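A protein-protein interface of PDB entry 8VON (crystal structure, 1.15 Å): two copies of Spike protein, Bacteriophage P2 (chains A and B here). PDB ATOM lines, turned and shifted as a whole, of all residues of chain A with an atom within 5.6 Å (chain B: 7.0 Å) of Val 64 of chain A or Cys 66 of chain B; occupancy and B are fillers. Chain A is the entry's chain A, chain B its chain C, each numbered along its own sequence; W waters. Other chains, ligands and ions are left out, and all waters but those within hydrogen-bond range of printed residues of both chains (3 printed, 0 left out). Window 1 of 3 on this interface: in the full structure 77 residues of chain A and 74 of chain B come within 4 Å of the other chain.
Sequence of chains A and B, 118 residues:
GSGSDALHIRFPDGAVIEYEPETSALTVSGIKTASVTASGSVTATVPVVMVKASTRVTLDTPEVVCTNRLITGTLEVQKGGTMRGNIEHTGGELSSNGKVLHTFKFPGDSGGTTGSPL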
ATOM      1  N   VAL A  57     -10.738  -0.039 -15.500  1.00  0.00           N
ATOM      2  CA  VAL A  57     -11.934  -0.196 -14.680  1.00  0.00           C
ATOM      3  C   VAL A  57     -11.531  -0.924 -13.413  1.00  0.00           C
ATOM      4  O   VAL A  57     -11.028  -2.048 -13.486  1.00  0.00           O
ATOM      5  CB  VAL A  57     -13.027  -1.002 -15.406  1.00  0.00           C
ATOM      6  CG1 VAL A  57     -14.214  -1.232 -14.493  1.00  0.00           C
ATOM      7  CG2 VAL A  57     -13.432  -0.306 -16.697  1.00  0.00           C
ATOM      8  N   LEU A  59     -12.972  -2.448  -9.836  1.00  0.00           N
ATOM      9  CA  LEU A  59     -14.107  -2.905  -9.036  1.00  0.00           C
ATOM     10  C   LEU A  59     -13.537  -3.224  -7.656  1.00  0.00           C
ATOM     11  O   LEU A  59     -12.989  -4.303  -7.437  1.00  0.00           O
ATOM     12  CB  LEU A  59     -14.783  -4.097  -9.700  1.00  0.00           C
ATOM     13  CG  LEU A  59     -15.219  -3.865 -11.138  1.00  0.00           C
ATOM     14  CD1 LEU A  59     -15.831  -5.133 -11.731  1.00  0.00           C
ATOM     15  CD2 LEU A  59     -16.152  -2.674 -11.283  1.00  0.00           C
ATOM     16  N   THR A  61     -14.189  -4.042  -4.224  1.00  0.00           N
ATOM     17  CA  THR A  61     -15.320  -4.634  -3.526  1.00  0.00           C
ATOM     18  C   THR A  61     -14.851  -5.955  -2.950  1.00  0.00           C
ATOM     19  O   THR A  61     -13.961  -6.601  -3.515  1.00  0.00           O
ATOM     20  CB  THR A  61     -16.501  -4.824  -4.504  1.00  0.00           C
ATOM     21  OG1 THR A  61     -17.636  -5.348  -3.836  1.00  0.00           O
ATOM     22  CG2 THR A  61     -16.184  -5.731  -5.660  1.00  0.00           C
ATOM     23  N   PRO A  62     -15.502  -6.451  -1.886  1.00  0.00           N
ATOM     24  CA  PRO A  62     -15.165  -7.805  -1.429  1.00  0.00           C
ATOM     25  C   PRO A  62     -15.411  -8.866  -2.474  1.00  0.00           C
ATOM     26  O   PRO A  62     -14.702  -9.884  -2.495  1.00  0.00           O
ATOM     27  CB  PRO A  62     -16.076  -7.990  -0.210  1.00  0.00           C
ATOM     28  CG  PRO A  62     -16.295  -6.601   0.306  1.00  0.00           C
ATOM     29  CD  PRO A  62     -16.397  -5.753  -0.929  1.00  0.00           C
ATOM     30  N   GLU A  63     -16.415  -8.679  -3.323  1.00  0.00           N
ATOM     31  CA  GLU A  63     -16.808  -9.707  -4.271  1.00  0.00           C
ATOM     32  C   GLU A  63     -17.450  -9.104  -5.498  1.00  0.00           C
ATOM     33  O   GLU A  63     -18.381  -8.304  -5.382  1.00  0.00           O
ATOM     34  CB  GLU A  63     -17.847 -10.572  -3.550  1.00  0.00           C
ATOM     35  CG  GLU A  63     -18.317 -11.820  -4.131  1.00  0.00           C
ATOM     36  CD  GLU A  63     -19.185 -12.510  -3.077  1.00  0.00           C
ATOM     37  OE1 GLU A  63     -18.590 -13.301  -2.369  1.00  0.00           O
ATOM     38  OE2 GLU A  63     -20.412 -12.260  -2.948  1.00  0.00           O
ATOM     39  N   VAL A  64     -16.940  -9.504  -6.658  1.00  0.00           N
ATOM     40  CA  VAL A  64     -17.574  -9.284  -7.946  1.00  0.00           C
ATOM     41  C   VAL A  64     -18.187 -10.618  -8.357  1.00  0.00           C
ATOM     42  O   VAL A  64     -17.493 -11.642  -8.375  1.00  0.00           O
ATOM     43  CB  VAL A  64     -16.558  -8.814  -9.000  1.00  0.00           C
ATOM     44  CG1 VAL A  64     -17.237  -8.685 -10.366  1.00  0.00           C
ATOM     45  CG2 VAL A  64     -15.886  -7.526  -8.603  1.00  0.00           C
ATOM     46  N   VAL A  65     -19.478 -10.610  -8.671  1.00  0.00           N
ATOM     47  CA  VAL A  65     -20.196 -11.808  -9.082  1.00  0.00           C
ATOM     48  C   VAL A  65     -20.643 -11.629 -10.519  1.00  0.00           C
ATOM     49  O   VAL A  65     -21.389 -10.697 -10.814  1.00  0.00           O
ATOM     50  CB  VAL A  65     -21.418 -12.078  -8.189  1.00  0.00           C
ATOM     51  CG1 VAL A  65     -22.200 -13.255  -8.729  1.00  0.00           C
ATOM     52  CG2 VAL A  65     -20.990 -12.267  -6.754  1.00  0.00           C
ATOM     53  N   CYS A  66     -20.186 -12.519 -11.398  1.00  0.00           N
ATOM     54  CA  CYS A  66     -20.709 -12.658 -12.751  1.00  0.00           C
ATOM     55  C   CYS A  66     -21.630 -13.877 -12.722  1.00  0.00           C
ATOM     56  O   CYS A  66     -21.180 -14.975 -12.400  1.00  0.00           O
ATOM     57  CB  CYS A  66     -19.591 -12.863 -13.765  1.00  0.00           C
ATOM     58  SG  CYS A  66     -18.356 -11.569 -13.740  1.00  0.00           S
ATOM     59  N   GLN A  78      -4.132 -13.296  -8.429  1.00  0.00           N
ATOM     60  CA  GLN A  78      -3.005 -12.906  -7.586  1.00  0.00           C
ATOM     61  C   GLN A  78      -2.824 -13.773  -6.350  1.00  0.00           C
ATOM     62  O   GLN A  78      -1.683 -13.952  -5.907  1.00  0.00           O
ATOM     63  CB  GLN A  78      -3.201 -11.462  -7.124  1.00  0.00           C
ATOM     64  CG  GLN A  78      -3.145 -10.447  -8.232  1.00  0.00           C
ATOM     65  CD  GLN A  78      -3.641  -9.079  -7.792  1.00  0.00           C
ATOM     66  OE1 GLN A  78      -4.596  -8.958  -6.993  1.00  0.00           O
ATOM     67  NE2 GLN A  78      -2.973  -8.040  -8.259  1.00  0.00           N
ATOM     68  N   VAL B  64      -9.266  -4.597 -16.329  1.00  0.00           N
ATOM     69  CA  VAL B  64     -10.283  -4.650 -15.295  1.00  0.00           C
ATOM     70  C   VAL B  64      -9.592  -5.218 -14.067  1.00  0.00           C
ATOM     71  O   VAL B  64      -8.968  -6.277 -14.148  1.00  0.00           O
ATOM     72  CB  VAL B  64     -11.456  -5.553 -15.710  1.00  0.00           C
ATOM     73  CG1 VAL B  64     -12.456  -5.658 -14.550  1.00  0.00           C
ATOM     74  CG2 VAL B  64     -12.106  -5.054 -16.969  1.00  0.00           C
ATOM     75  N   VAL B  65      -9.720  -4.537 -12.932  1.00  0.00           N
ATOM     76  CA  VAL B  65      -9.137  -4.977 -11.669  1.00  0.00           C
ATOM     77  C   VAL B  65     -10.259  -5.229 -10.667  1.00  0.00           C
ATOM     78  O   VAL B  65     -11.026  -4.321 -10.372  1.00  0.00           O
ATOM     79  CB  VAL B  65      -8.147  -3.947 -11.101  1.00  0.00           C
ATOM     80  CG1 VAL B  65      -7.653  -4.384  -9.731  1.00  0.00           C
ATOM     81  CG2 VAL B  65      -6.980  -3.735 -12.055  1.00  0.00           C
ATOM     82  N   CYS B  66     -10.349  -6.459 -10.156  1.00  0.00           N
ATOM     83  CA  CYS B  66     -11.207  -6.805  -9.029  1.00  0.00           C
ATOM     84  C   CYS B  66     -10.289  -6.917  -7.823  1.00  0.00           C
ATOM     85  O   CYS B  66      -9.339  -7.710  -7.838  1.00  0.00           O
ATOM     86  CB  CYS B  66     -11.924  -8.130  -9.283  1.00  0.00           C
ATOM     87  SG  CYS B  66     -12.892  -8.174 -10.780  1.00  0.00           S
ATOM     88  N   THR B  67     -10.544  -6.132  -6.784  1.00  0.00           N
ATOM     89  CA  THR B  67      -9.566  -6.022  -5.708  1.00  0.00           C
ATOM     90  C   THR B  67      -9.542  -7.214  -4.756  1.00  0.00           C
ATOM     91  O   THR B  67      -8.547  -7.364  -4.034  1.00  0.00           O
ATOM     92  CB  THR B  67      -9.754  -4.716  -4.937  1.00  0.00           C
ATOM     93  OG1 THR B  67     -11.066  -4.725  -4.399  1.00  0.00           O
ATOM     94  CG2 THR B  67      -9.507  -3.523  -5.827  1.00  0.00           C
ATOM     95  N   ASN B  68     -10.583  -8.028  -4.731  1.00  0.00           N
ATOM     96  CA  ASN B  68     -10.664  -9.168  -3.816  1.00  0.00           C
ATOM     97  C   ASN B  68     -11.161 -10.369  -4.606  1.00  0.00           C
ATOM     98  O   ASN B  68     -10.439 -10.847  -5.492  1.00  0.00           O
ATOM     99  CB  ASN B  68     -11.491  -8.821  -2.583  1.00  0.00           C
ATOM    100  CG  ASN B  68     -10.810  -7.773  -1.749  1.00  0.00           C
ATOM    101  OD1 ASN B  68      -9.881  -8.079  -0.998  1.00  0.00           O
ATOM    102  ND2 ASN B  68     -11.219  -6.537  -1.889  1.00  0.00           N
ATOM    103  N   ARG B  69     -12.370 -10.850  -4.333  1.00  0.00           N
ATOM    104  CA  ARG B  69     -12.871 -12.056  -4.964  1.00  0.00           C
ATOM    105  C   ARG B  69     -13.625 -11.761  -6.244  1.00  0.00           C
ATOM    106  O   ARG B  69     -14.343 -10.766  -6.333  1.00  0.00           O
ATOM    107  CB  ARG B  69     -13.826 -12.778  -4.024  1.00  0.00           C
ATOM    108  CG  ARG B  69     -14.303 -14.130  -4.503  1.00  0.00           C
ATOM    109  CD  ARG B  69     -14.842 -14.982  -3.373  1.00  0.00           C
ATOM    110  NE  ARG B  69     -15.751 -14.262  -2.504  1.00  0.00           N
ATOM    111  CZ  ARG B  69     -15.479 -13.895  -1.260  1.00  0.00           C
ATOM    112  NH1 ARG B  69     -14.297 -14.120  -0.712  1.00  0.00           N
ATOM    113  NH2 ARG B  69     -16.420 -13.289  -0.546  1.00  0.00           N
ATOM    114  N   LEU B  70     -13.469 -12.647  -7.219  1.00  0.00           N
ATOM    115  CA  LEU B  70     -14.255 -12.693  -8.435  1.00  0.00           C
ATOM    116  C   LEU B  70     -14.872 -14.079  -8.522  1.00  0.00           C
ATOM    117  O   LEU B  70     -14.158 -15.085  -8.433  1.00  0.00           O
ATOM    118  CB  LEU B  70     -13.354 -12.440  -9.631  1.00  0.00           C
ATOM    119  CG  LEU B  70     -13.966 -12.656 -10.997  1.00  0.00           C
ATOM    120  CD1 LEU B  70     -15.111 -11.720 -11.227  1.00  0.00           C
ATOM    121  CD2 LEU B  70     -12.895 -12.484 -12.046  1.00  0.00           C
ATOM    122  N   ILE B  71     -16.198 -14.127  -8.652  1.00  0.00           N
ATOM    123  CA  ILE B  71     -16.967 -15.356  -8.785  1.00  0.00           C
ATOM    124  C   ILE B  71     -17.628 -15.325 -10.149  1.00  0.00           C
ATOM    125  O   ILE B  71     -18.214 -14.303 -10.515  1.00  0.00           O
ATOM    126  CB  ILE B  71     -18.036 -15.476  -7.685  1.00  0.00           C
ATOM    127  CG1 ILE B  71     -17.401 -15.386  -6.297  1.00  0.00           C
ATOM    128  CG2 ILE B  71     -18.842 -16.748  -7.875  1.00  0.00           C
ATOM    129  CD1 ILE B  71     -18.445 -15.269  -5.178  1.00  0.00           C
ATOM    130  N   THR B  72     -17.551 -16.428 -10.885  1.00  0.00           N
ATOM    131  CA  THR B  72     -18.246 -16.529 -12.150  1.00  0.00           C
ATOM    132  C   THR B  72     -18.832 -17.929 -12.306  1.00  0.00           C
ATOM    133  O   THR B  72     -18.333 -18.903 -11.734  1.00  0.00           O
ATOM    134  CB  THR B  72     -17.326 -16.185 -13.340  1.00  0.00           C
ATOM    135  OG1 THR B  72     -18.128 -16.069 -14.509  1.00  0.00           O
ATOM    136  CG2 THR B  72     -16.206 -17.184 -13.536  1.00  0.00           C
HETATM  137  O   HOH W   1     -13.199  -4.017  -1.039  1.00  0.00           O
HETATM  138  O   HOH W   2     -13.235  -8.078  -5.876  1.00  0.00           O
HETATM  139  O   HOH W   3      -6.563  -7.351  -7.718  1.00  0.00           O
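The backbone carbonyl oxygen of Val 57 of chain A is in hydrogen-bond range of the backbone NH of Val 65 of chain B (2.9 Å). N of Leu 59 of chain A lies within hydrogen-bond range of O of Val 65 of chain B. The backbone NH of Thr 67 of chain B lies within hydrogen-bond range of the backbone carbonyl oxygen of Leu 59 of chain A (3.1 Å). The side-chain hydroxyl (OG1) of Thr 67 of chain B lies within hydrogen-bond range of the backbone NH (N) of Thr 61 of chain A, at 3.2 Å. The backbone carbonyl oxygen (O) of Thr 61 of chain A lies within hydrogen-bond range of the side-chain amide nitrogen (ND2) of Asn 68 of chain B. O of Pro 62 of chain A is in hydrogen-bond range of N of Arg 69 of chain B, 3.1 Å away. OE1 of Glu 63 of chain A lies within salt-bridge range of NH2 of Arg 69 of chain B, at 2.8 Å. The backbone NH (N) of Val 64 of chain A lies within hydrogen-bond range of the backbone carbonyl oxygen (O) of Arg 69 of chain B. The backbone carbonyl oxygen (O) of Val 64 of chain A sits at hydrogen-bond distance from the backbone NH (N) of Ile 71 of chain B (2.8 Å). The backbone NH of Cys 66 of chain A lies within hydrogen-bond range of the backbone carbonyl oxygen of Ile 71 of chain B (2.8 Å).
OG1 of Thr 61 of chain A sits close to O of Glu 63 of chain A (3.4 Å). The side-chain hydroxyl (OG1) of Thr 67 of chain B lies within hydrogen-bond range of the side-chain amide nitrogen (ND2) of Asn 68 of chain B, at 3.1 Å.
O of Val 57 of chain A touches CA of Val 64 of chain B (3.3 Å). Cys 66 of chain B touches Leu 59 of chain A (CA to O, 3.5 Å). Asn 68 of chain B touches Pro 62 of chain A. Glu 63 of chain A touches Ile 71 of chain B (OE1 to CD1, 3.4 Å). Val 64 of chain A touches Cys 66 of chain B (CG2 to SG, 3.8 Å). Val 64 of chain A touches Leu 70 of chain B. Ile 71 of chain B touches Val 65 of chain A (O to CA, 3.5 Å). Cys 66 of chain A touches Thr 72 of chain B (O to CA, 3.3 Å).
Val 64 of chain A touches just these residues of chain B: Cys 66, Arg 69, Leu 70 and Ile 71. Cys 66 of chain B touches two residues of chain A. Printed residues of chain A within 4 Å of Val 64 of chain B: Val 57. Of the printed residues of chain A, Val 65 of chain B touches Val 57 and Leu 59. Printed residues of chain A within 4 Å of Leu 70 of chain B: Val 64 (3.4 Å). Printed residues of chain A within 4 Å of Thr 72 of chain B: Cys 66 (3.3 Å).
Printed residues of chain A that touch a printed residue of chain B: Val 57, Leu 59, Thr 61, Pro 62, Glu 63, Val 64, Val 65 and Cys 66. Hydrophobic or aromatic side chains of chain A that line the printed part of chain B: Leu 59 and Val 64. Hydrophobic or aromatic side chains of chain B that line the printed part of chain A: Leu 70 and Ile 71. Among the printed residues, 18 pairs touch across the chains. Among the printed residues, Asp or Glu carboxylates within 4 Å of a Lys or Arg side-chain nitrogen of the other chain: Glu 63 of chain A with Arg 69 of chain B.
Val 64 of chain A touches Cys 66 of chain B, but with the chains exchanged Cys 66 of chain A does not touch Val 64 of chain B (8.4 Å). Positions printed for both chains: 64, 65 and 66.
Water W3 lies within hydrogen-bond range of the side-chain amide oxygen (OE1) of Gln 78 of chain A and the backbone carbonyl oxygen (O) of Cys 66 of chain B. Water W2 lies within hydrogen-bond range of O of Thr 61 of chain A (2.9 Å), N of Asn 68 of chain B (2.9 Å), O of Arg 69 of chain B (2.9 Å) and N of Thr 67 of chain B (3.4 Å). Water W1 bridges ND2 of Asn 68 of chain B (3.3 Å) and N of Thr 61 of chain A (3.3 Å).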
